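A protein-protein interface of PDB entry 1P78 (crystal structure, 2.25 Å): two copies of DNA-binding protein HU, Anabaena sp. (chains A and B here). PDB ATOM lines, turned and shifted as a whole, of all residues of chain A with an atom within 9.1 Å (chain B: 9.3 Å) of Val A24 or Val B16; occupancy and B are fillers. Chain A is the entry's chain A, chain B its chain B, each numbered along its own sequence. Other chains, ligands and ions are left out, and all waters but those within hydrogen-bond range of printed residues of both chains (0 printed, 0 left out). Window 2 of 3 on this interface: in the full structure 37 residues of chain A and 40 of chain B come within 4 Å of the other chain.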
ATOM      1  N   LYS A   3      32.176  -7.792 -17.874  1.00  0.00           N
ATOM      2  CA  LYS A   3      30.733  -7.697 -17.701  1.00  0.00           C
ATOM      3  C   LYS A   3      30.021  -8.004 -19.023  1.00  0.00           C
ATOM      4  O   LYS A   3      29.200  -8.919 -19.104  1.00  0.00           O
ATOM      5  CB  LYS A   3      30.347  -6.311 -17.178  1.00  0.00           C
ATOM      6  CG  LYS A   3      28.886  -6.187 -16.768  1.00  0.00           C
ATOM      7  CD  LYS A   3      28.603  -4.854 -16.091  1.00  0.00           C
ATOM      8  CE  LYS A   3      27.116  -4.652 -15.903  1.00  0.00           C
ATOM      9  NZ  LYS A   3      26.769  -3.212 -15.825  1.00  0.00           N
ATOM     10  N   VAL A   7      27.441 -10.942 -19.899  1.00  0.00           N
ATOM     11  CA  VAL A   7      26.089 -10.635 -20.397  1.00  0.00           C
ATOM     12  C   VAL A   7      25.765 -11.437 -21.669  1.00  0.00           C
ATOM     13  O   VAL A   7      24.718 -12.086 -21.752  1.00  0.00           O
ATOM     14  CB  VAL A   7      25.883  -9.115 -20.656  1.00  0.00           C
ATOM     15  CG1 VAL A   7      24.441  -8.819 -21.048  1.00  0.00           C
ATOM     16  CG2 VAL A   7      26.274  -8.294 -19.441  1.00  0.00           C
ATOM     17  N   VAL A  10      25.255 -15.123 -20.943  1.00  0.00           N
ATOM     18  CA  VAL A  10      24.059 -15.291 -20.133  1.00  0.00           C
ATOM     19  C   VAL A  10      22.796 -15.250 -20.996  1.00  0.00           C
ATOM     20  O   VAL A  10      21.947 -16.143 -20.920  1.00  0.00           O
ATOM     21  CB  VAL A  10      24.001 -14.185 -19.063  1.00  0.00           C
ATOM     22  CG1 VAL A  10      22.667 -14.198 -18.325  1.00  0.00           C
ATOM     23  CG2 VAL A  10      25.183 -14.326 -18.099  1.00  0.00           C
ATOM     24  N   ALA A  14      19.920 -18.518 -20.671  1.00  0.00           N
ATOM     25  CA  ALA A  14      18.585 -18.292 -20.111  1.00  0.00           C
ATOM     26  C   ALA A  14      17.629 -17.845 -21.201  1.00  0.00           C
ATOM     27  O   ALA A  14      16.419 -18.114 -21.139  1.00  0.00           O
ATOM     28  CB  ALA A  14      18.644 -17.247 -19.005  1.00  0.00           C
ATOM     29  N   VAL A  16      17.497 -14.285 -23.271  1.00  0.00           N
ATOM     30  CA  VAL A  16      16.974 -12.918 -23.175  1.00  0.00           C
ATOM     31  C   VAL A  16      17.815 -11.997 -24.088  1.00  0.00           C
ATOM     32  O   VAL A  16      18.543 -12.487 -24.963  1.00  0.00           O
ATOM     33  CB  VAL A  16      17.004 -12.395 -21.713  1.00  0.00           C
ATOM     34  CG1 VAL A  16      16.075 -13.218 -20.807  1.00  0.00           C
ATOM     35  CG2 VAL A  16      18.435 -12.411 -21.178  1.00  0.00           C
ATOM     36  N   THR A  17      17.721 -10.679 -23.885  1.00  0.00           N
ATOM     37  CA  THR A  17      18.534  -9.715 -24.642  1.00  0.00           C
ATOM     38  C   THR A  17      19.783  -9.267 -23.906  1.00  0.00           C
ATOM     39  O   THR A  17      19.822  -9.299 -22.682  1.00  0.00           O
ATOM     40  CB  THR A  17      17.732  -8.463 -24.942  1.00  0.00           C
ATOM     41  OG1 THR A  17      16.343  -8.731 -24.685  1.00  0.00           O
ATOM     42  CG2 THR A  17      17.807  -8.143 -26.451  1.00  0.00           C
ATOM     43  N   LYS A  18      20.778  -8.813 -24.679  1.00  0.00           N
ATOM     44  CA  LYS A  18      21.974  -8.133 -24.162  1.00  0.00           C
ATOM     45  C   LYS A  18      21.603  -6.950 -23.255  1.00  0.00           C
ATOM     46  O   LYS A  18      21.997  -6.913 -22.098  1.00  0.00           O
ATOM     47  CB  LYS A  18      22.876  -7.661 -25.317  1.00  0.00           C
ATOM     48  CG  LYS A  18      23.813  -8.744 -25.906  1.00  0.00           C
ATOM     49  CD  LYS A  18      24.822  -8.106 -26.896  1.00  0.00           C
ATOM     50  CE  LYS A  18      25.761  -9.149 -27.496  1.00  0.00           C
ATOM     51  NZ  LYS A  18      26.923  -8.520 -28.194  1.00  0.00           N
ATOM     52  N   LYS A  19      20.827  -6.000 -23.778  1.00  0.00           N
ATOM     53  CA  LYS A  19      20.276  -4.918 -22.957  1.00  0.00           C
ATOM     54  C   LYS A  19      19.574  -5.450 -21.692  1.00  0.00           C
ATOM     55  O   LYS A  19      19.713  -4.877 -20.604  1.00  0.00           O
ATOM     56  CB  LYS A  19      19.299  -4.063 -23.775  1.00  0.00           C
ATOM     57  CG  LYS A  19      18.982  -2.717 -23.119  1.00  0.00           C
ATOM     58  CD  LYS A  19      17.776  -2.012 -23.766  1.00  0.00           C
ATOM     59  CE  LYS A  19      17.567  -0.602 -23.167  1.00  0.00           C
ATOM     60  NZ  LYS A  19      16.649   0.282 -23.975  1.00  0.00           N
ATOM     61  N   GLN A  20      18.831  -6.548 -21.866  1.00  0.00           N
ATOM     62  CA  GLN A  20      18.002  -7.171 -20.835  1.00  0.00           C
ATOM     63  C   GLN A  20      18.867  -7.796 -19.773  1.00  0.00           C
ATOM     64  O   GLN A  20      18.873  -7.365 -18.622  1.00  0.00           O
ATOM     65  CB  GLN A  20      17.138  -8.248 -21.485  1.00  0.00           C
ATOM     66  CG  GLN A  20      16.100  -8.927 -20.602  1.00  0.00           C
ATOM     67  CD  GLN A  20      14.776  -9.164 -21.361  1.00  0.00           C
ATOM     68  OE1 GLN A  20      14.059  -8.208 -21.682  1.00  0.00           O
ATOM     69  NE2 GLN A  20      14.464 -10.434 -21.656  1.00  0.00           N
ATOM     70  N   ALA A  21      19.610  -8.819 -20.184  1.00  0.00           N
ATOM     71  CA  ALA A  21      20.543  -9.537 -19.321  1.00  0.00           C
ATOM     72  C   ALA A  21      21.483  -8.584 -18.602  1.00  0.00           C
ATOM     73  O   ALA A  21      21.800  -8.794 -17.417  1.00  0.00           O
ATOM     74  CB  ALA A  21      21.352 -10.553 -20.137  1.00  0.00           C
ATOM     75  N   ASP A  22      21.945  -7.557 -19.315  1.00  0.00           N
ATOM     76  CA  ASP A  22      22.765  -6.545 -18.684  1.00  0.00           C
ATOM     77  C   ASP A  22      21.963  -5.898 -17.554  1.00  0.00           C
ATOM     78  O   ASP A  22      22.366  -5.944 -16.393  1.00  0.00           O
ATOM     79  CB  ASP A  22      23.248  -5.483 -19.679  1.00  0.00           C
ATOM     80  CG  ASP A  22      24.028  -4.368 -18.983  1.00  0.00           C
ATOM     81  OD1 ASP A  22      23.353  -3.391 -18.509  1.00  0.00           O
ATOM     82  OD2 ASP A  22      25.290  -4.396 -18.820  1.00  0.00           O
ATOM     83  N   ALA A  23      20.816  -5.324 -17.892  1.00  0.00           N
ATOM     84  CA  ALA A  23      19.988  -4.684 -16.884  1.00  0.00           C
ATOM     85  C   ALA A  23      19.810  -5.564 -15.636  1.00  0.00           C
ATOM     86  O   ALA A  23      19.874  -5.067 -14.503  1.00  0.00           O
ATOM     87  CB  ALA A  23      18.625  -4.282 -17.476  1.00  0.00           C
ATOM     88  N   VAL A  24      19.591  -6.861 -15.848  1.00  0.00           N
ATOM     89  CA  VAL A  24      19.310  -7.771 -14.739  1.00  0.00           C
ATOM     90  C   VAL A  24      20.567  -8.078 -13.913  1.00  0.00           C
ATOM     91  O   VAL A  24      20.534  -8.010 -12.680  1.00  0.00           O
ATOM     92  CB  VAL A  24      18.641  -9.094 -15.199  1.00  0.00           C
ATOM     93  CG1 VAL A  24      18.247  -9.971 -14.000  1.00  0.00           C
ATOM     94  CG2 VAL A  24      17.427  -8.830 -16.058  1.00  0.00           C
ATOM     95  N   LEU A  25      21.674  -8.400 -14.578  1.00  0.00           N
ATOM     96  CA  LEU A  25      22.907  -8.703 -13.843  1.00  0.00           C
ATOM     97  C   LEU A  25      23.275  -7.519 -12.939  1.00  0.00           C
ATOM     98  O   LEU A  25      23.560  -7.710 -11.761  1.00  0.00           O
ATOM     99  CB  LEU A  25      24.058  -9.089 -14.782  1.00  0.00           C
ATOM    100  CG  LEU A  25      25.462  -9.156 -14.159  1.00  0.00           C
ATOM    101  CD1 LEU A  25      25.700 -10.441 -13.350  1.00  0.00           C
ATOM    102  CD2 LEU A  25      26.555  -8.954 -15.206  1.00  0.00           C
ATOM    103  N   THR A  26      23.218  -6.313 -13.511  1.00  0.00           N
ATOM    104  CA  THR A  26      23.418  -5.033 -12.818  1.00  0.00           C
ATOM    105  C   THR A  26      22.543  -4.883 -11.569  1.00  0.00           C
ATOM    106  O   THR A  26      23.050  -4.672 -10.460  1.00  0.00           O
ATOM    107  CB  THR A  26      23.151  -3.871 -13.807  1.00  0.00           C
ATOM    108  OG1 THR A  26      24.262  -3.750 -14.709  1.00  0.00           O
ATOM    109  CG2 THR A  26      23.095  -2.521 -13.098  1.00  0.00           C
ATOM    110  N   ALA A  27      21.233  -4.988 -11.752  1.00  0.00           N
ATOM    111  CA  ALA A  27      20.311  -4.992 -10.623  1.00  0.00           C
ATOM    112  C   ALA A  27      20.873  -5.831  -9.473  1.00  0.00           C
ATOM    113  O   ALA A  27      20.926  -5.375  -8.332  1.00  0.00           O
ATOM    114  CB  ALA A  27      18.952  -5.526 -11.051  1.00  0.00           C
ATOM    115  N   ALA A  28      21.313  -7.045  -9.796  1.00  0.00           N
ATOM    116  CA  ALA A  28      21.843  -7.981  -8.810  1.00  0.00           C
ATOM    117  C   ALA A  28      23.149  -7.492  -8.181  1.00  0.00           C
ATOM    118  O   ALA A  28      23.320  -7.583  -6.971  1.00  0.00           O
ATOM    119  CB  ALA A  28      22.035  -9.368  -9.454  1.00  0.00           C
ATOM    120  N   LEU A  29      24.059  -6.977  -9.009  1.00  0.00           N
ATOM    121  CA  LEU A  29      25.353  -6.497  -8.520  1.00  0.00           C
ATOM    122  C   LEU A  29      25.215  -5.318  -7.581  1.00  0.00           C
ATOM    123  O   LEU A  29      25.904  -5.265  -6.563  1.00  0.00           O
ATOM    124  CB  LEU A  29      26.312  -6.133  -9.667  1.00  0.00           C
ATOM    125  CG  LEU A  29      26.786  -7.249 -10.614  1.00  0.00           C
ATOM    126  CD1 LEU A  29      27.900  -6.730 -11.544  1.00  0.00           C
ATOM    127  CD2 LEU A  29      27.218  -8.523  -9.870  1.00  0.00           C
ATOM    128  N   GLU A  30      24.336  -4.380  -7.936  1.00  0.00           N
ATOM    129  CA  GLU A  30      24.077  -3.201  -7.111  1.00  0.00           C
ATOM    130  C   GLU A  30      23.337  -3.559  -5.813  1.00  0.00           C
ATOM    131  O   GLU A  30      23.631  -3.006  -4.740  1.00  0.00           O
ATOM    132  CB  GLU A  30      23.296  -2.153  -7.897  1.00  0.00           C
ATOM    133  CG  GLU A  30      23.966  -1.688  -9.185  1.00  0.00           C
ATOM    134  CD  GLU A  30      23.107  -0.674  -9.953  1.00  0.00           C
ATOM    135  OE1 GLU A  30      21.862  -0.618  -9.726  1.00  0.00           O
ATOM    136  OE2 GLU A  30      23.680   0.073 -10.795  1.00  0.00           O
ATOM    137  N   THR A  31      22.399  -4.499  -5.918  1.00  0.00           N
ATOM    138  CA  THR A  31      21.704  -5.058  -4.755  1.00  0.00           C
ATOM    139  C   THR A  31      22.629  -5.799  -3.799  1.00  0.00           C
ATOM    140  O   THR A  31      22.495  -5.661  -2.576  1.00  0.00           O
ATOM    141  CB  THR A  31      20.575  -5.997  -5.197  1.00  0.00           C
ATOM    142  OG1 THR A  31      19.678  -5.276  -6.039  1.00  0.00           O
ATOM    143  CG2 THR A  31      19.708  -6.428  -4.016  1.00  0.00           C
ATOM    144  N   ILE A  32      23.552  -6.590  -4.348  1.00  0.00           N
ATOM    145  CA  ILE A  32      24.543  -7.282  -3.529  1.00  0.00           C
ATOM    146  C   ILE A  32      25.310  -6.265  -2.662  1.00  0.00           C
ATOM    147  O   ILE A  32      25.306  -6.370  -1.426  1.00  0.00           O
ATOM    148  CB  ILE A  32      25.489  -8.155  -4.408  1.00  0.00           C
ATOM    149  CG1 ILE A  32      24.743  -9.406  -4.911  1.00  0.00           C
ATOM    150  CG2 ILE A  32      26.753  -8.575  -3.624  1.00  0.00           C
ATOM    151  CD1 ILE A  32      25.510 -10.216  -5.913  1.00  0.00           C
ATOM    152  N   LEU B   6      17.200 -12.250  -3.411  1.00  0.00           N
ATOM    153  CA  LEU B   6      17.909 -11.499  -4.438  1.00  0.00           C
ATOM    154  C   LEU B   6      17.132 -11.546  -5.754  1.00  0.00           C
ATOM    155  O   LEU B   6      16.983 -10.522  -6.428  1.00  0.00           O
ATOM    156  CB  LEU B   6      19.351 -12.041  -4.619  1.00  0.00           C
ATOM    157  CG  LEU B   6      20.196 -11.336  -5.685  1.00  0.00           C
ATOM    158  CD1 LEU B   6      20.524  -9.921  -5.270  1.00  0.00           C
ATOM    159  CD2 LEU B   6      21.480 -12.096  -6.017  1.00  0.00           C
ATOM    160  N   VAL B   7      16.635 -12.732  -6.108  1.00  0.00           N
ATOM    161  CA  VAL B   7      15.805 -12.880  -7.303  1.00  0.00           C
ATOM    162  C   VAL B   7      14.609 -11.940  -7.205  1.00  0.00           C
ATOM    163  O   VAL B   7      14.397 -11.126  -8.116  1.00  0.00           O
ATOM    164  CB  VAL B   7      15.301 -14.335  -7.539  1.00  0.00           C
ATOM    165  CG1 VAL B   7      14.222 -14.365  -8.640  1.00  0.00           C
ATOM    166  CG2 VAL B   7      16.468 -15.286  -7.889  1.00  0.00           C
ATOM    167  N   ASP B   8      13.855 -12.027  -6.101  1.00  0.00           N
ATOM    168  CA  ASP B   8      12.637 -11.211  -5.938  1.00  0.00           C
ATOM    169  C   ASP B   8      12.949  -9.732  -6.134  1.00  0.00           C
ATOM    170  O   ASP B   8      12.287  -9.049  -6.910  1.00  0.00           O
ATOM    171  CB  ASP B   8      11.991 -11.435  -4.564  1.00  0.00           C
ATOM    172  CG  ASP B   8      11.468 -12.856  -4.378  1.00  0.00           C
ATOM    173  OD1 ASP B   8      11.630 -13.697  -5.292  1.00  0.00           O
ATOM    174  OD2 ASP B   8      10.873 -13.226  -3.345  1.00  0.00           O
ATOM    175  N   ALA B   9      13.999  -9.273  -5.451  1.00  0.00           N
ATOM    176  CA  ALA B   9      14.443  -7.881  -5.495  1.00  0.00           C
ATOM    177  C   ALA B   9      14.922  -7.458  -6.880  1.00  0.00           C
ATOM    178  O   ALA B   9      14.681  -6.326  -7.309  1.00  0.00           O
ATOM    179  CB  ALA B   9      15.550  -7.670  -4.474  1.00  0.00           C
ATOM    180  N   VAL B  10      15.610  -8.375  -7.557  1.00  0.00           N
ATOM    181  CA  VAL B  10      16.161  -8.141  -8.893  1.00  0.00           C
ATOM    182  C   VAL B  10      15.067  -8.032  -9.965  1.00  0.00           C
ATOM    183  O   VAL B  10      15.107  -7.138 -10.825  1.00  0.00           O
ATOM    184  CB  VAL B  10      17.191  -9.238  -9.267  1.00  0.00           C
ATOM    185  CG1 VAL B  10      17.596  -9.135 -10.736  1.00  0.00           C
ATOM    186  CG2 VAL B  10      18.429  -9.132  -8.359  1.00  0.00           C
ATOM    187  N   ALA B  11      14.089  -8.932  -9.904  1.00  0.00           N
ATOM    188  CA  ALA B  11      12.992  -8.950 -10.878  1.00  0.00           C
ATOM    189  C   ALA B  11      12.389  -7.554 -11.032  1.00  0.00           C
ATOM    190  O   ALA B  11      12.051  -7.123 -12.142  1.00  0.00           O
ATOM    191  CB  ALA B  11      11.914  -9.970 -10.470  1.00  0.00           C
ATOM    192  N   GLU B  12      12.291  -6.853  -9.904  1.00  0.00           N
ATOM    193  CA  GLU B  12      11.642  -5.556  -9.832  1.00  0.00           C
ATOM    194  C   GLU B  12      12.500  -4.445 -10.452  1.00  0.00           C
ATOM    195  O   GLU B  12      12.055  -3.767 -11.383  1.00  0.00           O
ATOM    196  CB  GLU B  12      11.304  -5.238  -8.373  1.00  0.00           C
ATOM    197  CG  GLU B  12      10.294  -6.198  -7.718  1.00  0.00           C
ATOM    198  CD  GLU B  12       9.654  -5.577  -6.483  1.00  0.00           C
ATOM    199  OE1 GLU B  12      10.388  -4.780  -5.770  1.00  0.00           O
ATOM    200  OE2 GLU B  12       8.410  -5.861  -6.235  1.00  0.00           O
ATOM    201  N   LYS B  13      13.723  -4.280  -9.945  1.00  0.00           N
ATOM    202  CA  LYS B  13      14.633  -3.199 -10.361  1.00  0.00           C
ATOM    203  C   LYS B  13      14.821  -3.080 -11.885  1.00  0.00           C
ATOM    204  O   LYS B  13      14.786  -1.974 -12.428  1.00  0.00           O
ATOM    205  CB  LYS B  13      16.013  -3.366  -9.685  1.00  0.00           C
ATOM    206  CG  LYS B  13      16.041  -3.127  -8.168  1.00  0.00           C
ATOM    207  CD  LYS B  13      17.489  -3.047  -7.605  1.00  0.00           C
ATOM    208  CE  LYS B  13      17.473  -2.639  -6.101  1.00  0.00           C
ATOM    209  NZ  LYS B  13      18.836  -2.418  -5.463  1.00  0.00           N
ATOM    210  N   ALA B  14      15.033  -4.217 -12.562  1.00  0.00           N
ATOM    211  CA  ALA B  14      15.331  -4.225 -14.001  1.00  0.00           C
ATOM    212  C   ALA B  14      14.081  -4.438 -14.868  1.00  0.00           C
ATOM    213  O   ALA B  14      14.128  -4.264 -16.102  1.00  0.00           O
ATOM    214  CB  ALA B  14      16.383  -5.288 -14.322  1.00  0.00           C
ATOM    215  N   SER B  15      12.987  -4.821 -14.195  1.00  0.00           N
ATOM    216  CA  SER B  15      11.699  -5.160 -14.818  1.00  0.00           C
ATOM    217  C   SER B  15      11.666  -6.504 -15.593  1.00  0.00           C
ATOM    218  O   SER B  15      11.579  -6.510 -16.839  1.00  0.00           O
ATOM    219  CB  SER B  15      11.131  -3.993 -15.671  1.00  0.00           C
ATOM    220  OG  SER B  15      10.739  -2.878 -14.854  1.00  0.00           O
ATOM    221  N   VAL B  16      11.717  -7.628 -14.843  1.00  0.00           N
ATOM    222  CA  VAL B  16      11.470  -8.974 -15.406  1.00  0.00           C
ATOM    223  C   VAL B  16      10.556  -9.849 -14.514  1.00  0.00           C
ATOM    224  O   VAL B  16       9.865  -9.324 -13.607  1.00  0.00           O
ATOM    225  CB  VAL B  16      12.792  -9.735 -15.751  1.00  0.00           C
ATOM    226  CG1 VAL B  16      13.632  -8.956 -16.770  1.00  0.00           C
ATOM    227  CG2 VAL B  16      13.602 -10.039 -14.496  1.00  0.00           C
ATOM    228  N   THR B  17      10.546 -11.170 -14.787  1.00  0.00           N
ATOM    229  CA  THR B  17       9.781 -12.149 -14.006  1.00  0.00           C
ATOM    230  C   THR B  17      10.678 -12.812 -12.973  1.00  0.00           C
ATOM    231  O   THR B  17      11.905 -12.737 -13.088  1.00  0.00           O
ATOM    232  CB  THR B  17       9.217 -13.241 -14.926  1.00  0.00           C
ATOM    233  OG1 THR B  17       9.592 -12.938 -16.286  1.00  0.00           O
ATOM    234  CG2 THR B  17       7.660 -13.181 -14.963  1.00  0.00           C
ATOM    235  N   LYS B  18      10.071 -13.482 -11.988  1.00  0.00           N
ATOM    236  CA  LYS B  18      10.824 -14.222 -10.959  1.00  0.00           C
ATOM    237  C   LYS B  18      11.467 -15.514 -11.515  1.00  0.00           C
ATOM    238  O   LYS B  18      12.603 -15.856 -11.153  1.00  0.00           O
ATOM    239  CB  LYS B  18       9.942 -14.524  -9.728  1.00  0.00           C
ATOM    240  CG  LYS B  18       9.648 -13.294  -8.839  1.00  0.00           C
ATOM    241  CD  LYS B  18       9.045 -13.645  -7.463  1.00  0.00           C
ATOM    242  CE  LYS B  18       8.727 -12.358  -6.660  1.00  0.00           C
ATOM    243  NZ  LYS B  18       8.276 -12.609  -5.259  1.00  0.00           N
ATOM    244  N   LYS B  19      10.740 -16.221 -12.393  1.00  0.00           N
ATOM    245  CA  LYS B  19      11.294 -17.384 -13.091  1.00  0.00           C
ATOM    246  C   LYS B  19      12.388 -16.949 -14.080  1.00  0.00           C
ATOM    247  O   LYS B  19      13.392 -17.659 -14.280  1.00  0.00           O
ATOM    248  N   GLN B  20      12.169 -15.776 -14.682  1.00  0.00           N
ATOM    249  CA  GLN B  20      13.091 -15.140 -15.623  1.00  0.00           C
ATOM    250  C   GLN B  20      14.375 -14.714 -14.929  1.00  0.00           C
ATOM    251  O   GLN B  20      15.419 -15.344 -15.128  1.00  0.00           O
ATOM    252  CB  GLN B  20      12.406 -13.931 -16.270  1.00  0.00           C
ATOM    253  CG  GLN B  20      13.071 -13.357 -17.540  1.00  0.00           C
ATOM    254  CD  GLN B  20      12.049 -12.720 -18.485  1.00  0.00           C
ATOM    255  OE1 GLN B  20      11.323 -13.429 -19.174  1.00  0.00           O
ATOM    256  NE2 GLN B  20      11.997 -11.390 -18.515  1.00  0.00           N
ATOM    257  N   ALA B  21      14.296 -13.672 -14.096  1.00  0.00           N
ATOM    258  CA  ALA B  21      15.459 -13.150 -13.363  1.00  0.00           C
ATOM    259  C   ALA B  21      16.330 -14.244 -12.775  1.00  0.00           C
ATOM    260  O   ALA B  21      17.559 -14.192 -12.902  1.00  0.00           O
ATOM    261  CB  ALA B  21      15.027 -12.194 -12.246  1.00  0.00           C
ATOM    262  N   ASP B  22      15.687 -15.214 -12.119  1.00  0.00           N
ATOM    263  CA  ASP B  22      16.383 -16.356 -11.539  1.00  0.00           C
ATOM    264  C   ASP B  22      17.254 -17.047 -12.587  1.00  0.00           C
ATOM    265  O   ASP B  22      18.467 -17.184 -12.414  1.00  0.00           O
ATOM    266  CB  ASP B  22      15.391 -17.372 -10.970  1.00  0.00           C
ATOM    267  CG  ASP B  22      16.085 -18.624 -10.481  1.00  0.00           C
ATOM    268  OD1 ASP B  22      16.594 -19.392 -11.340  1.00  0.00           O
ATOM    269  OD2 ASP B  22      16.219 -18.903  -9.264  1.00  0.00           O
ATOM    270  N   ALA B  23      16.621 -17.477 -13.673  1.00  0.00           N
ATOM    271  CA  ALA B  23      17.321 -18.149 -14.762  1.00  0.00           C
ATOM    272  C   ALA B  23      18.517 -17.333 -15.255  1.00  0.00           C
ATOM    273  O   ALA B  23      19.556 -17.902 -15.590  1.00  0.00           O
ATOM    274  CB  ALA B  23      16.342 -18.456 -15.933  1.00  0.00           C
ATOM    275  N   VAL B  24      18.353 -16.008 -15.298  1.00  0.00           N
ATOM    276  CA  VAL B  24      19.427 -15.087 -15.686  1.00  0.00           C
ATOM    277  C   VAL B  24      20.551 -15.089 -14.645  1.00  0.00           C
ATOM    278  O   VAL B  24      21.697 -15.374 -14.958  1.00  0.00           O
ATOM    279  CB  VAL B  24      18.919 -13.628 -15.822  1.00  0.00           C
ATOM    280  CG1 VAL B  24      20.076 -12.652 -16.158  1.00  0.00           C
ATOM    281  CG2 VAL B  24      17.805 -13.528 -16.828  1.00  0.00           C
ATOM    282  N   LEU B  25      20.203 -14.759 -13.408  1.00  0.00           N
ATOM    283  CA  LEU B  25      21.171 -14.713 -12.337  1.00  0.00           C
ATOM    284  C   LEU B  25      21.957 -16.036 -12.279  1.00  0.00           C
ATOM    285  O   LEU B  25      23.197 -16.031 -12.139  1.00  0.00           O
ATOM    286  CB  LEU B  25      20.469 -14.406 -11.011  1.00  0.00           C
ATOM    287  CG  LEU B  25      21.340 -14.458  -9.745  1.00  0.00           C
ATOM    288  CD1 LEU B  25      22.329 -13.269  -9.648  1.00  0.00           C
ATOM    289  CD2 LEU B  25      20.468 -14.591  -8.476  1.00  0.00           C
ATOM    290  N   THR B  26      21.229 -17.145 -12.413  1.00  0.00           N
ATOM    291  CA  THR B  26      21.810 -18.481 -12.450  1.00  0.00           C
ATOM    292  C   THR B  26      22.862 -18.585 -13.561  1.00  0.00           C
ATOM    293  O   THR B  26      24.028 -18.896 -13.299  1.00  0.00           O
ATOM    294  CB  THR B  26      20.697 -19.555 -12.655  1.00  0.00           C
ATOM    295  OG1 THR B  26      19.943 -19.720 -11.446  1.00  0.00           O
ATOM    296  CG2 THR B  26      21.290 -20.930 -12.868  1.00  0.00           C
ATOM    297  N   ALA B  28      24.580 -16.396 -15.087  1.00  0.00           N
ATOM    298  CA  ALA B  28      25.747 -15.614 -14.724  1.00  0.00           C
ATOM    299  C   ALA B  28      26.623 -16.304 -13.677  1.00  0.00           C
ATOM    300  O   ALA B  28      27.845 -16.237 -13.765  1.00  0.00           O
ATOM    301  CB  ALA B  28      25.327 -14.227 -14.260  1.00  0.00           C
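The side-chain hydroxyl (OG1) of Thr A31 sits at hydrogen-bond distance from the side-chain amino group (NZ) of Lys B13 (3.0 Å).
N of Val B16 lies within hydrogen-bond range of O of Ala B11 (2.8 Å).
The side-chain hydroxyl (OG1) of Thr A31 lies within hydrogen-bond range of the backbone carbonyl oxygen (O) of Ala A27 (2.6 Å).
Val A10 touches Val B24.
O of Ala B23 touches CB of Ala A14 (3.6 Å).
Val B24 touches Ala A14.
Val A24 touches Val B16 (CG2 to CG1, 3.9 Å).
Val A24 touches Val B24.
Leu A25 touches Ala B28.
CB of Ala A27 touches CG1 of Val B10 (3.9 Å).
Lys B13 touches Ala A27 (CB to CB, 3.9 Å).
Ala A28 touches Leu B25.
CD1 of Leu B6 touches CG2 of Thr A31 (3.8 Å).
Printed residues of chain B within 4 Å of Val A10: Val B24 (3.7 Å) and Ala B28 (3.7 Å).
Of the printed residues of chain B, Ala A14 touches Ala B23 (3.6 Å) and Val B24 (3.9 Å).
Val A16 touches none of the printed residues of chain B.
Lys A19 touches none of the printed residues of chain B.
Of chain B, only Ala B14 (3.5 Å) comes within 4 Å of Ala A23.
Of chain B, only Val B10 (3.4 Å), Ala B14 (3.9 Å), Val B16 (3.9 Å) and Val B24 (3.9 Å) come within 4 Å of Val A24.
Of the printed residues of chain B, Ala A27 touches Val B10 (3.9 Å) and Lys B13 (3.9 Å).
Of the printed residues of chain B, Thr A31 touches Leu B6 (3.8 Å) and Lys B13 (3.0 Å).
No residue of chain A comes within 4 Å of Ser B15.
Of chain A, only Val A24 (3.9 Å) comes within 4 Å of Val B16.
No residue of chain A comes within 4 Å of Thr B17.
No residue of chain A comes within 4 Å of Ala B21.
The nearest residue of chain A that does not touch Val B16 is Gln A20 (4.6 Å).
The nearest printed residue of chain A that does not touch Ala B28 is Val A7 (6.9 Å).
Of the 21 printed residues of chain A, 8 touch a printed residue of chain B.
Hydrophobic or aromatic side chains of chain A within 4 Å of the printed part of chain B: Val A10, Ala A14, Ala A23, Val A24, Leu A25, Ala A27 and Ala A28.
Of the 22 printed residues of chain B, 9 touch a printed residue of chain A.
Among the printed residues, 16 pairs touch across the chains.
Val A10 touches Ala B28, and with the chains exchanged Ala A28 touches Val B10.
Ala A14 touches Ala B23, and with the chains exchanged Ala A23 touches Ala B14.
Ala A14 touches Val B24, and with the chains exchanged Val A24 touches Ala B14.
Leu A25 touches Ala B28, and with the chains exchanged Ala A28 touches Leu B25.
15 positions are printed for both chains.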
